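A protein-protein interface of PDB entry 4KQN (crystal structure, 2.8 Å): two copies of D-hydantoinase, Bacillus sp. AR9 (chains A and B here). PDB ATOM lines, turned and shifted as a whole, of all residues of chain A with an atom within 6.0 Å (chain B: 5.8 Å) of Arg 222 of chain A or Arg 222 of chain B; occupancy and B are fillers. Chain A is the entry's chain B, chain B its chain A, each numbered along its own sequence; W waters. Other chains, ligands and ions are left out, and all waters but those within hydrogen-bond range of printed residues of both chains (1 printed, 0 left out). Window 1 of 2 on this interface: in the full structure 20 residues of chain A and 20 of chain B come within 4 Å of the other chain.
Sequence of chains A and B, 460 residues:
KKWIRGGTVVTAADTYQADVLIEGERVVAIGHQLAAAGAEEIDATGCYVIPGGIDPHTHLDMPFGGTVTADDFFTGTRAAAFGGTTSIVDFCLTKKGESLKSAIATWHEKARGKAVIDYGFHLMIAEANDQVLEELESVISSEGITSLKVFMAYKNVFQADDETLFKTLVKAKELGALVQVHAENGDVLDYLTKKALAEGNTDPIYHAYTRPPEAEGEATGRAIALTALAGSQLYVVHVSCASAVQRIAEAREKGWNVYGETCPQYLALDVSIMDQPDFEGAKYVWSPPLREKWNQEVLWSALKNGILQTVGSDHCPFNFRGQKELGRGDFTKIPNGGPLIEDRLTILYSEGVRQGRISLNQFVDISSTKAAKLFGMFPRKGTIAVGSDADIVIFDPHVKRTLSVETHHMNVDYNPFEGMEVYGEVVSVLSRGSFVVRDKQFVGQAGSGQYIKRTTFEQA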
ATOM      1  N   MET A 152       2.366  30.262 -12.119  1.00  0.00           N
ATOM      2  CA  MET A 152       2.646  29.298 -13.165  1.00  0.00           C
ATOM      3  C   MET A 152       3.028  27.964 -12.577  1.00  0.00           C
ATOM      4  O   MET A 152       3.257  26.998 -13.327  1.00  0.00           O
ATOM      5  CB  MET A 152       3.738  29.819 -14.082  1.00  0.00           C
ATOM      6  CG  MET A 152       3.251  31.008 -14.875  1.00  0.00           C
ATOM      7  SD  MET A 152       4.577  31.980 -15.515  1.00  0.00           S
ATOM      8  CE  MET A 152       4.912  31.101 -17.023  1.00  0.00           C
ATOM      9  N   ASP A 162      -1.242  28.740 -19.854  1.00  0.00           N
ATOM     10  CA  ASP A 162      -0.810  29.853 -20.727  1.00  0.00           C
ATOM     11  C   ASP A 162      -2.025  30.675 -21.177  1.00  0.00           C
ATOM     12  O   ASP A 162      -1.950  31.885 -21.277  1.00  0.00           O
ATOM     13  CB  ASP A 162       0.008  29.350 -21.943  1.00  0.00           C
ATOM     14  CG  ASP A 162       1.410  28.771 -21.570  1.00  0.00           C
ATOM     15  OD1 ASP A 162       2.117  29.363 -20.719  1.00  0.00           O
ATOM     16  OD2 ASP A 162       1.823  27.745 -22.166  1.00  0.00           O
ATOM     17  N   LEU A 165      -3.078  32.944 -18.349  1.00  0.00           N
ATOM     18  CA  LEU A 165      -1.923  33.850 -18.404  1.00  0.00           C
ATOM     19  C   LEU A 165      -2.091  34.914 -19.526  1.00  0.00           C
ATOM     20  O   LEU A 165      -2.198  36.101 -19.234  1.00  0.00           O
ATOM     21  CB  LEU A 165      -0.598  33.052 -18.528  1.00  0.00           C
ATOM     22  CG  LEU A 165       0.677  33.548 -17.781  1.00  0.00           C
ATOM     23  CD1 LEU A 165       1.982  32.907 -18.272  1.00  0.00           C
ATOM     24  CD2 LEU A 165       0.860  35.048 -17.834  1.00  0.00           C
ATOM     25  N   GLU A 184       7.659  29.611 -12.249  1.00  0.00           N
ATOM     26  CA  GLU A 184       8.297  28.296 -12.299  1.00  0.00           C
ATOM     27  C   GLU A 184       7.379  27.352 -13.053  1.00  0.00           C
ATOM     28  O   GLU A 184       6.175  27.471 -12.936  1.00  0.00           O
ATOM     29  CB  GLU A 184       8.514  27.743 -10.898  1.00  0.00           C
ATOM     30  CG  GLU A 184       9.469  28.545 -10.056  1.00  0.00           C
ATOM     31  CD  GLU A 184      10.045  27.733  -8.917  1.00  0.00           C
ATOM     32  OE1 GLU A 184       9.304  27.578  -7.906  1.00  0.00           O
ATOM     33  OE2 GLU A 184      11.229  27.259  -9.059  1.00  0.00           O
ATOM     34  N   ASN A 185       7.929  26.414 -13.801  1.00  0.00           N
ATOM     35  CA  ASN A 185       7.094  25.535 -14.574  1.00  0.00           C
ATOM     36  C   ASN A 185       6.537  24.433 -13.713  1.00  0.00           C
ATOM     37  O   ASN A 185       7.190  23.382 -13.534  1.00  0.00           O
ATOM     38  CB  ASN A 185       7.866  24.910 -15.729  1.00  0.00           C
ATOM     39  CG  ASN A 185       6.962  24.142 -16.677  1.00  0.00           C
ATOM     40  OD1 ASN A 185       6.102  23.362 -16.262  1.00  0.00           O
ATOM     41  ND2 ASN A 185       7.139  24.375 -17.949  1.00  0.00           N
ATOM     42  N   GLY A 186       5.335  24.669 -13.183  1.00  0.00           N
ATOM     43  CA  GLY A 186       4.588  23.651 -12.444  1.00  0.00           C
ATOM     44  C   GLY A 186       4.786  22.255 -12.992  1.00  0.00           C
ATOM     45  O   GLY A 186       5.250  21.369 -12.292  1.00  0.00           O
ATOM     46  N   ASP A 187       4.485  22.046 -14.262  1.00  0.00           N
ATOM     47  CA  ASP A 187       4.488  20.690 -14.796  1.00  0.00           C
ATOM     48  C   ASP A 187       5.802  19.959 -14.535  1.00  0.00           C
ATOM     49  O   ASP A 187       5.782  18.846 -14.058  1.00  0.00           O
ATOM     50  CB  ASP A 187       4.117  20.702 -16.281  1.00  0.00           C
ATOM     51  CG  ASP A 187       2.769  21.407 -16.551  1.00  0.00           C
ATOM     52  OD1 ASP A 187       1.726  20.836 -16.214  1.00  0.00           O
ATOM     53  OD2 ASP A 187       2.742  22.517 -17.097  1.00  0.00           O
ATOM     54  N   GLY A 217      14.005  30.002 -15.071  1.00  0.00           N
ATOM     55  CA  GLY A 217      14.449  30.631 -16.287  1.00  0.00           C
ATOM     56  C   GLY A 217      13.416  30.462 -17.369  1.00  0.00           C
ATOM     57  O   GLY A 217      13.124  31.383 -18.107  1.00  0.00           O
ATOM     58  N   GLU A 218      12.847  29.279 -17.430  1.00  0.00           N
ATOM     59  CA  GLU A 218      11.927  28.964 -18.478  1.00  0.00           C
ATOM     60  C   GLU A 218      10.613  29.730 -18.334  1.00  0.00           C
ATOM     61  O   GLU A 218      10.175  30.376 -19.267  1.00  0.00           O
ATOM     62  CB  GLU A 218      11.702  27.452 -18.523  1.00  0.00           C
ATOM     63  CG  GLU A 218      10.877  27.004 -19.702  1.00  0.00           C
ATOM     64  CD  GLU A 218       9.429  27.395 -19.597  1.00  0.00           C
ATOM     65  OE1 GLU A 218       8.833  27.166 -18.532  1.00  0.00           O
ATOM     66  OE2 GLU A 218       8.895  27.947 -20.588  1.00  0.00           O
ATOM     67  N   ALA A 219       9.999  29.671 -17.164  1.00  0.00           N
ATOM     68  CA  ALA A 219       8.695  30.322 -16.966  1.00  0.00           C
ATOM     69  C   ALA A 219       8.810  31.797 -17.065  1.00  0.00           C
ATOM     70  O   ALA A 219       7.907  32.454 -17.541  1.00  0.00           O
ATOM     71  CB  ALA A 219       8.106  29.955 -15.627  1.00  0.00           C
ATOM     72  N   THR A 220       9.945  32.325 -16.629  1.00  0.00           N
ATOM     73  CA  THR A 220      10.220  33.747 -16.747  1.00  0.00           C
ATOM     74  C   THR A 220      10.259  34.149 -18.227  1.00  0.00           C
ATOM     75  O   THR A 220       9.596  35.091 -18.621  1.00  0.00           O
ATOM     76  CB  THR A 220      11.539  34.071 -16.056  1.00  0.00           C
ATOM     77  OG1 THR A 220      11.471  33.596 -14.720  1.00  0.00           O
ATOM     78  CG2 THR A 220      11.787  35.544 -16.006  1.00  0.00           C
ATOM     79  N   GLY A 221      11.006  33.414 -19.032  1.00  0.00           N
ATOM     80  CA  GLY A 221      11.120  33.679 -20.432  1.00  0.00           C
ATOM     81  C   GLY A 221       9.759  33.654 -21.047  1.00  0.00           C
ATOM     82  O   GLY A 221       9.395  34.529 -21.844  1.00  0.00           O
ATOM     83  N   ARG A 222       9.000  32.637 -20.649  1.00  0.00           N
ATOM     84  CA  ARG A 222       7.673  32.377 -21.187  1.00  0.00           C
ATOM     85  C   ARG A 222       6.745  33.522 -20.893  1.00  0.00           C
ATOM     86  O   ARG A 222       6.086  34.034 -21.802  1.00  0.00           O
ATOM     87  CB  ARG A 222       7.098  31.092 -20.601  1.00  0.00           C
ATOM     88  CG  ARG A 222       5.647  30.791 -21.002  1.00  0.00           C
ATOM     89  CD  ARG A 222       5.448  29.287 -21.166  1.00  0.00           C
ATOM     90  NE  ARG A 222       6.029  28.495 -20.069  1.00  0.00           N
ATOM     91  CZ  ARG A 222       5.357  28.106 -18.987  1.00  0.00           C
ATOM     92  NH1 ARG A 222       4.092  28.445 -18.849  1.00  0.00           N
ATOM     93  NH2 ARG A 222       5.940  27.382 -18.048  1.00  0.00           N
ATOM     94  N   ALA A 223       6.702  33.921 -19.636  1.00  0.00           N
ATOM     95  CA  ALA A 223       5.762  34.961 -19.210  1.00  0.00           C
ATOM     96  C   ALA A 223       6.115  36.281 -19.864  1.00  0.00           C
ATOM     97  O   ALA A 223       5.236  37.078 -20.183  1.00  0.00           O
ATOM     98  CB  ALA A 223       5.783  35.104 -17.701  1.00  0.00           C
ATOM     99  N   ILE A 224       7.411  36.484 -20.113  1.00  0.00           N
ATOM    100  CA  ILE A 224       7.865  37.650 -20.877  1.00  0.00           C
ATOM    101  C   ILE A 224       7.400  37.627 -22.337  1.00  0.00           C
ATOM    102  O   ILE A 224       7.033  38.660 -22.902  1.00  0.00           O
ATOM    103  CB  ILE A 224       9.380  37.737 -20.849  1.00  0.00           C
ATOM    104  CG1 ILE A 224       9.828  38.239 -19.469  1.00  0.00           C
ATOM    105  CG2 ILE A 224       9.890  38.686 -21.916  1.00  0.00           C
ATOM    106  CD1 ILE A 224      11.257  37.875 -19.067  1.00  0.00           C
ATOM    107  N   ALA A 225       7.403  36.447 -22.943  1.00  0.00           N
ATOM    108  CA  ALA A 225       7.083  36.358 -24.333  1.00  0.00           C
ATOM    109  C   ALA A 225       5.622  36.747 -24.564  1.00  0.00           C
ATOM    110  O   ALA A 225       5.323  37.542 -25.476  1.00  0.00           O
ATOM    111  CB  ALA A 225       7.381  34.972 -24.846  1.00  0.00           C
ATOM    112  N   LEU A 226       4.720  36.255 -23.713  1.00  0.00           N
ATOM    113  CA  LEU A 226       3.293  36.627 -23.827  1.00  0.00           C
ATOM    114  C   LEU A 226       3.060  38.126 -23.640  1.00  0.00           C
ATOM    115  O   LEU A 226       2.377  38.787 -24.452  1.00  0.00           O
ATOM    116  CB  LEU A 226       2.437  35.850 -22.835  1.00  0.00           C
ATOM    117  CG  LEU A 226       2.728  34.342 -22.818  1.00  0.00           C
ATOM    118  CD1 LEU A 226       1.658  33.612 -22.034  1.00  0.00           C
ATOM    119  CD2 LEU A 226       2.817  33.762 -24.219  1.00  0.00           C
ATOM    120  N   THR A 227       3.624  38.660 -22.564  1.00  0.00           N
ATOM    121  CA  THR A 227       3.667  40.097 -22.345  1.00  0.00           C
ATOM    122  C   THR A 227       4.040  40.834 -23.655  1.00  0.00           C
ATOM    123  O   THR A 227       3.358  41.772 -24.064  1.00  0.00           O
ATOM    124  CB  THR A 227       4.675  40.389 -21.235  1.00  0.00           C
ATOM    125  OG1 THR A 227       4.431  39.460 -20.174  1.00  0.00           O
ATOM    126  CG2 THR A 227       4.559  41.825 -20.695  1.00  0.00           C
ATOM    127  N   ARG A 247      16.891  36.580 -18.657  1.00  0.00           N
ATOM    128  CA  ARG A 247      15.718  36.717 -19.487  1.00  0.00           C
ATOM    129  C   ARG A 247      15.056  38.099 -19.321  1.00  0.00           C
ATOM    130  O   ARG A 247      14.539  38.671 -20.304  1.00  0.00           O
ATOM    131  CB  ARG A 247      14.693  35.603 -19.156  1.00  0.00           C
ATOM    132  CG  ARG A 247      14.565  34.485 -20.194  1.00  0.00           C
ATOM    133  CD  ARG A 247      15.871  33.736 -20.377  1.00  0.00           C
ATOM    134  NE  ARG A 247      15.902  32.855 -21.562  1.00  0.00           N
ATOM    135  CZ  ARG A 247      16.912  32.788 -22.439  1.00  0.00           C
ATOM    136  NH1 ARG A 247      18.004  33.557 -22.300  1.00  0.00           N
ATOM    137  NH2 ARG A 247      16.843  31.945 -23.474  1.00  0.00           N
ATOM    138  N   MET B 152       3.100  21.085 -29.886  1.00  0.00           N
ATOM    139  CA  MET B 152       2.818  22.039 -28.839  1.00  0.00           C
ATOM    140  C   MET B 152       1.674  22.951 -29.256  1.00  0.00           C
ATOM    141  O   MET B 152       1.240  23.801 -28.466  1.00  0.00           O
ATOM    142  CB  MET B 152       4.085  22.831 -28.475  1.00  0.00           C
ATOM    143  CG  MET B 152       5.138  21.959 -27.845  1.00  0.00           C
ATOM    144  SD  MET B 152       6.781  22.665 -27.928  1.00  0.00           S
ATOM    145  CE  MET B 152       6.744  23.689 -26.492  1.00  0.00           C
ATOM    146  N   ASP B 162       2.983  20.500 -21.219  1.00  0.00           N
ATOM    147  CA  ASP B 162       4.377  20.449 -20.826  1.00  0.00           C
ATOM    148  C   ASP B 162       4.661  19.119 -20.117  1.00  0.00           C
ATOM    149  O   ASP B 162       5.720  18.522 -20.296  1.00  0.00           O
ATOM    150  CB  ASP B 162       4.751  21.635 -19.941  1.00  0.00           C
ATOM    151  CG  ASP B 162       4.747  22.978 -20.692  1.00  0.00           C
ATOM    152  OD1 ASP B 162       5.329  23.069 -21.784  1.00  0.00           O
ATOM    153  OD2 ASP B 162       4.177  23.970 -20.172  1.00  0.00           O
ATOM    154  N   LEU B 165       5.038  16.449 -22.824  1.00  0.00           N
ATOM    155  CA  LEU B 165       6.341  16.903 -23.353  1.00  0.00           C
ATOM    156  C   LEU B 165       7.537  16.428 -22.479  1.00  0.00           C
ATOM    157  O   LEU B 165       8.353  15.622 -22.926  1.00  0.00           O
ATOM    158  CB  LEU B 165       6.346  18.434 -23.547  1.00  0.00           C
ATOM    159  CG  LEU B 165       7.059  19.050 -24.770  1.00  0.00           C
ATOM    160  CD1 LEU B 165       7.308  20.556 -24.645  1.00  0.00           C
ATOM    161  CD2 LEU B 165       8.385  18.397 -25.077  1.00  0.00           C
ATOM    162  N   GLU B 184       5.048  25.769 -31.461  1.00  0.00           N
ATOM    163  CA  GLU B 184       4.270  27.012 -31.394  1.00  0.00           C
ATOM    164  C   GLU B 184       3.352  26.898 -30.215  1.00  0.00           C
ATOM    165  O   GLU B 184       2.859  25.833 -29.924  1.00  0.00           O
ATOM    166  CB  GLU B 184       3.423  27.207 -32.645  1.00  0.00           C
ATOM    167  CG  GLU B 184       4.212  27.399 -33.923  1.00  0.00           C
ATOM    168  CD  GLU B 184       3.411  28.089 -35.009  1.00  0.00           C
ATOM    169  OE1 GLU B 184       2.607  27.379 -35.654  1.00  0.00           O
ATOM    170  OE2 GLU B 184       3.637  29.325 -35.197  1.00  0.00           O
ATOM    171  N   ASN B 185       3.089  28.004 -29.549  1.00  0.00           N
ATOM    172  CA  ASN B 185       2.247  27.964 -28.377  1.00  0.00           C
ATOM    173  C   ASN B 185       0.795  27.947 -28.783  1.00  0.00           C
ATOM    174  O   ASN B 185       0.174  29.006 -28.926  1.00  0.00           O
ATOM    175  CB  ASN B 185       2.505  29.170 -27.473  1.00  0.00           C
ATOM    176  CG  ASN B 185       1.815  29.036 -26.140  1.00  0.00           C
ATOM    177  OD1 ASN B 185       0.639  28.679 -26.059  1.00  0.00           O
ATOM    178  ND2 ASN B 185       2.543  29.305 -25.081  1.00  0.00           N
ATOM    179  N   GLY B 186       0.255  26.736 -28.938  1.00  0.00           N
ATOM    180  CA  GLY B 186      -1.194  26.528 -29.115  1.00  0.00           C
ATOM    181  C   GLY B 186      -2.063  27.554 -28.386  1.00  0.00           C
ATOM    182  O   GLY B 186      -2.819  28.277 -29.000  1.00  0.00           O
ATOM    183  N   GLY B 217       9.285  31.271 -31.193  1.00  0.00           N
ATOM    184  CA  GLY B 217      10.439  31.550 -30.388  1.00  0.00           C
ATOM    185  C   GLY B 217      10.188  30.989 -29.017  1.00  0.00           C
ATOM    186  O   GLY B 217      11.067  30.391 -28.418  1.00  0.00           O
ATOM    187  N   GLU B 218       8.977  31.199 -28.522  1.00  0.00           N
ATOM    188  CA  GLU B 218       8.672  30.856 -27.158  1.00  0.00           C
ATOM    189  C   GLU B 218       8.640  29.348 -26.979  1.00  0.00           C
ATOM    190  O   GLU B 218       9.284  28.820 -26.091  1.00  0.00           O
ATOM    191  CB  GLU B 218       7.364  31.513 -26.745  1.00  0.00           C
ATOM    192  CG  GLU B 218       7.048  31.328 -25.286  1.00  0.00           C
ATOM    193  CD  GLU B 218       6.645  29.899 -24.966  1.00  0.00           C
ATOM    194  OE1 GLU B 218       5.774  29.341 -25.682  1.00  0.00           O
ATOM    195  OE2 GLU B 218       7.207  29.326 -23.998  1.00  0.00           O
ATOM    196  N   ALA B 219       7.912  28.646 -27.834  1.00  0.00           N
ATOM    197  CA  ALA B 219       7.782  27.204 -27.676  1.00  0.00           C
ATOM    198  C   ALA B 219       9.099  26.508 -27.905  1.00  0.00           C
ATOM    199  O   ALA B 219       9.388  25.504 -27.293  1.00  0.00           O
ATOM    200  CB  ALA B 219       6.719  26.643 -28.608  1.00  0.00           C
ATOM    201  N   THR B 220       9.876  27.025 -28.828  1.00  0.00           N
ATOM    202  CA  THR B 220      11.201  26.464 -29.117  1.00  0.00           C
ATOM    203  C   THR B 220      12.078  26.570 -27.894  1.00  0.00           C
ATOM    204  O   THR B 220      12.650  25.593 -27.480  1.00  0.00           O
ATOM    205  CB  THR B 220      11.834  27.227 -30.282  1.00  0.00           C
ATOM    206  OG1 THR B 220      10.930  27.190 -31.385  1.00  0.00           O
ATOM    207  CG2 THR B 220      13.116  26.628 -30.695  1.00  0.00           C
ATOM    208  N   GLY B 221      12.118  27.757 -27.285  1.00  0.00           N
ATOM    209  CA  GLY B 221      12.847  27.983 -26.062  1.00  0.00           C
ATOM    210  C   GLY B 221      12.412  27.037 -24.974  1.00  0.00           C
ATOM    211  O   GLY B 221      13.232  26.433 -24.297  1.00  0.00           O
ATOM    212  N   ARG B 222      11.099  26.894 -24.851  1.00  0.00           N
ATOM    213  CA  ARG B 222      10.478  26.072 -23.832  1.00  0.00           C
ATOM    214  C   ARG B 222      10.873  24.665 -23.991  1.00  0.00           C
ATOM    215  O   ARG B 222      11.315  24.029 -23.042  1.00  0.00           O
ATOM    216  CB  ARG B 222       8.968  26.182 -23.933  1.00  0.00           C
ATOM    217  CG  ARG B 222       8.205  25.255 -22.998  1.00  0.00           C
ATOM    218  CD  ARG B 222       6.918  25.924 -22.479  1.00  0.00           C
ATOM    219  NE  ARG B 222       6.134  26.622 -23.516  1.00  0.00           N
ATOM    220  CZ  ARG B 222       5.185  26.051 -24.227  1.00  0.00           C
ATOM    221  NH1 ARG B 222       4.873  24.779 -24.016  1.00  0.00           N
ATOM    222  NH2 ARG B 222       4.527  26.739 -25.137  1.00  0.00           N
ATOM    223  N   ALA B 223      10.727  24.170 -25.211  1.00  0.00           N
ATOM    224  CA  ALA B 223      11.013  22.756 -25.490  1.00  0.00           C
ATOM    225  C   ALA B 223      12.498  22.460 -25.249  1.00  0.00           C
ATOM    226  O   ALA B 223      12.865  21.358 -24.831  1.00  0.00           O
ATOM    227  CB  ALA B 223      10.627  22.379 -26.913  1.00  0.00           C
ATOM    228  N   ILE B 224      13.341  23.450 -25.517  1.00  0.00           N
ATOM    229  CA  ILE B 224      14.748  23.319 -25.238  1.00  0.00           C
ATOM    230  C   ILE B 224      15.002  23.214 -23.732  1.00  0.00           C
ATOM    231  O   ILE B 224      15.904  22.480 -23.286  1.00  0.00           O
ATOM    232  CB  ILE B 224      15.519  24.507 -25.840  1.00  0.00           C
ATOM    233  CG1 ILE B 224      15.652  24.309 -27.364  1.00  0.00           C
ATOM    234  CG2 ILE B 224      16.885  24.639 -25.220  1.00  0.00           C
ATOM    235  CD1 ILE B 224      15.878  25.577 -28.164  1.00  0.00           C
ATOM    236  N   ALA B 225      14.258  23.979 -22.947  1.00  0.00           N
ATOM    237  CA  ALA B 225      14.552  24.059 -21.545  1.00  0.00           C
ATOM    238  C   ALA B 225      14.286  22.708 -20.905  1.00  0.00           C
ATOM    239  O   ALA B 225      15.133  22.214 -20.124  1.00  0.00           O
ATOM    240  CB  ALA B 225      13.746  25.147 -20.899  1.00  0.00           C
ATOM    241  N   LEU B 226      13.171  22.062 -21.273  1.00  0.00           N
ATOM    242  CA  LEU B 226      12.868  20.710 -20.721  1.00  0.00           C
ATOM    243  C   LEU B 226      13.919  19.665 -21.102  1.00  0.00           C
ATOM    244  O   LEU B 226      14.438  18.937 -20.260  1.00  0.00           O
ATOM    245  CB  LEU B 226      11.497  20.253 -21.169  1.00  0.00           C
ATOM    246  CG  LEU B 226      10.409  21.309 -21.000  1.00  0.00           C
ATOM    247  CD1 LEU B 226       9.050  20.679 -21.225  1.00  0.00           C
ATOM    248  CD2 LEU B 226      10.451  21.961 -19.637  1.00  0.00           C
ATOM    249  N   THR B 227      14.250  19.630 -22.387  1.00  0.00           N
ATOM    250  CA  THR B 227      15.378  18.848 -22.903  1.00  0.00           C
ATOM    251  C   THR B 227      16.631  19.001 -22.004  1.00  0.00           C
ATOM    252  O   THR B 227      17.223  18.041 -21.572  1.00  0.00           O
ATOM    253  CB  THR B 227      15.667  19.294 -24.362  1.00  0.00           C
ATOM    254  OG1 THR B 227      14.432  19.405 -25.065  1.00  0.00           O
ATOM    255  CG2 THR B 227      16.596  18.303 -25.125  1.00  0.00           C
HETATM  256  O   HOH W   1       2.894  25.926 -20.834  1.00  0.00           O
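ND2 of Asn 185 of chain B sits at hydrogen-bond distance from OD2 of Asp 162 of chain A, 3.4 Å away.
The side-chain carboxylate of Asp 162 of chain B lies within salt-bridge range of the guanidinium group of Arg 222 of chain B, at 2.8 Å. OE1 of Glu 218 of chain B lies within hydrogen-bond range of ND2 of Asn 185 of chain B (3.3 Å). The side-chain carboxylate (OE1) of Glu 218 of chain B is in salt-bridge range of the guanidinium group (NH2) of Arg 222 of chain B. The side-chain amide oxygen of Asn 185 of chain A is in hydrogen-bond range of the backbone NH of Asp 187 of chain A, 2.9 Å away. ND2 of Asn 185 of chain A lies close to NH2 of Arg 222 of chain A. NH2 of Arg 222 of chain A is in salt-bridge range of OE1 of Glu 218 of chain A (2.9 Å).
Asn 185 of chain A touches Asp 162 of chain B (ND2 to OD2, 3.7 Å). Asp 162 of chain B touches Asp 187 of chain A (CB to OD2, 3.6 Å). Glu 218 of chain A touches Arg 222 of chain B. Ala 225 of chain B touches Glu 218 of chain A (CB to CG, 3.6 Å). OE2 of Glu 218 of chain B touches CD of Arg 222 of chain A, at 3.3 Å. CD of Arg 222 of chain A touches NE of Arg 222 of chain B (3.6 Å). Ala 225 of chain A touches Glu 218 of chain B.
Of the printed residues of chain B, Arg 222 of chain A touches Glu 218 and Arg 222. Of chain A, only Glu 218 (3.4 Å) and Arg 222 (3.6 Å) come within 4 Å of Arg 222 of chain B. Of the printed residues of chain A, Asp 162 of chain B touches Asn 185 (3.7 Å) and Asp 187 (3.6 Å). Of the printed residues of chain B, Asp 187 of chain A touches Asp 162. Printed residues of chain B within 4 Å of Asn 185 of chain A: Asp 162. The nearest residue of chain B that does not touch Arg 222 of chain A is Asp 162 of chain B (4.4 Å).
Printed residues of chain B that touch a printed residue of chain A: Asp 162, Asn 185, Glu 218, Arg 222 and Ala 225. Hydrophobic or aromatic side chains of chain B within 4 Å of the printed part of chain A: Ala 225. Along chain A the printed residues that touch a printed residue of chain B span positions 162 to 225. Among the printed residues, no Asp or Glu carboxylate lies within 4 Å of a Lys or Arg side-chain nitrogen of the other chain.
Asp 162 of chain A touches Asn 185 of chain B, and with the chains exchanged Asn 185 of chain A touches Asp 162 of chain B. Glu 218 of chain A touches Arg 222 of chain B, and with the chains exchanged Arg 222 of chain A touches Glu 218 of chain B. Glu 218 of chain A touches Ala 225 of chain B, and with the chains exchanged Ala 225 of chain A touches Glu 218 of chain B. Arg 222 of chain B touches its own counterpart, Arg 222 of chain A. Positions printed for both chains: 152, 162, 165, 184, 185, 186, 217, 218, 219, 220, 221, 222, 223, 224, 225, 226 and 227.
Water W1 lies within hydrogen-bond range of OD2 of Asp 162 of chain B (2.4 Å), OD2 of Asp 162 of chain A (2.5 Å) and NH1 of Arg 222 of chain A (3.4 Å).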
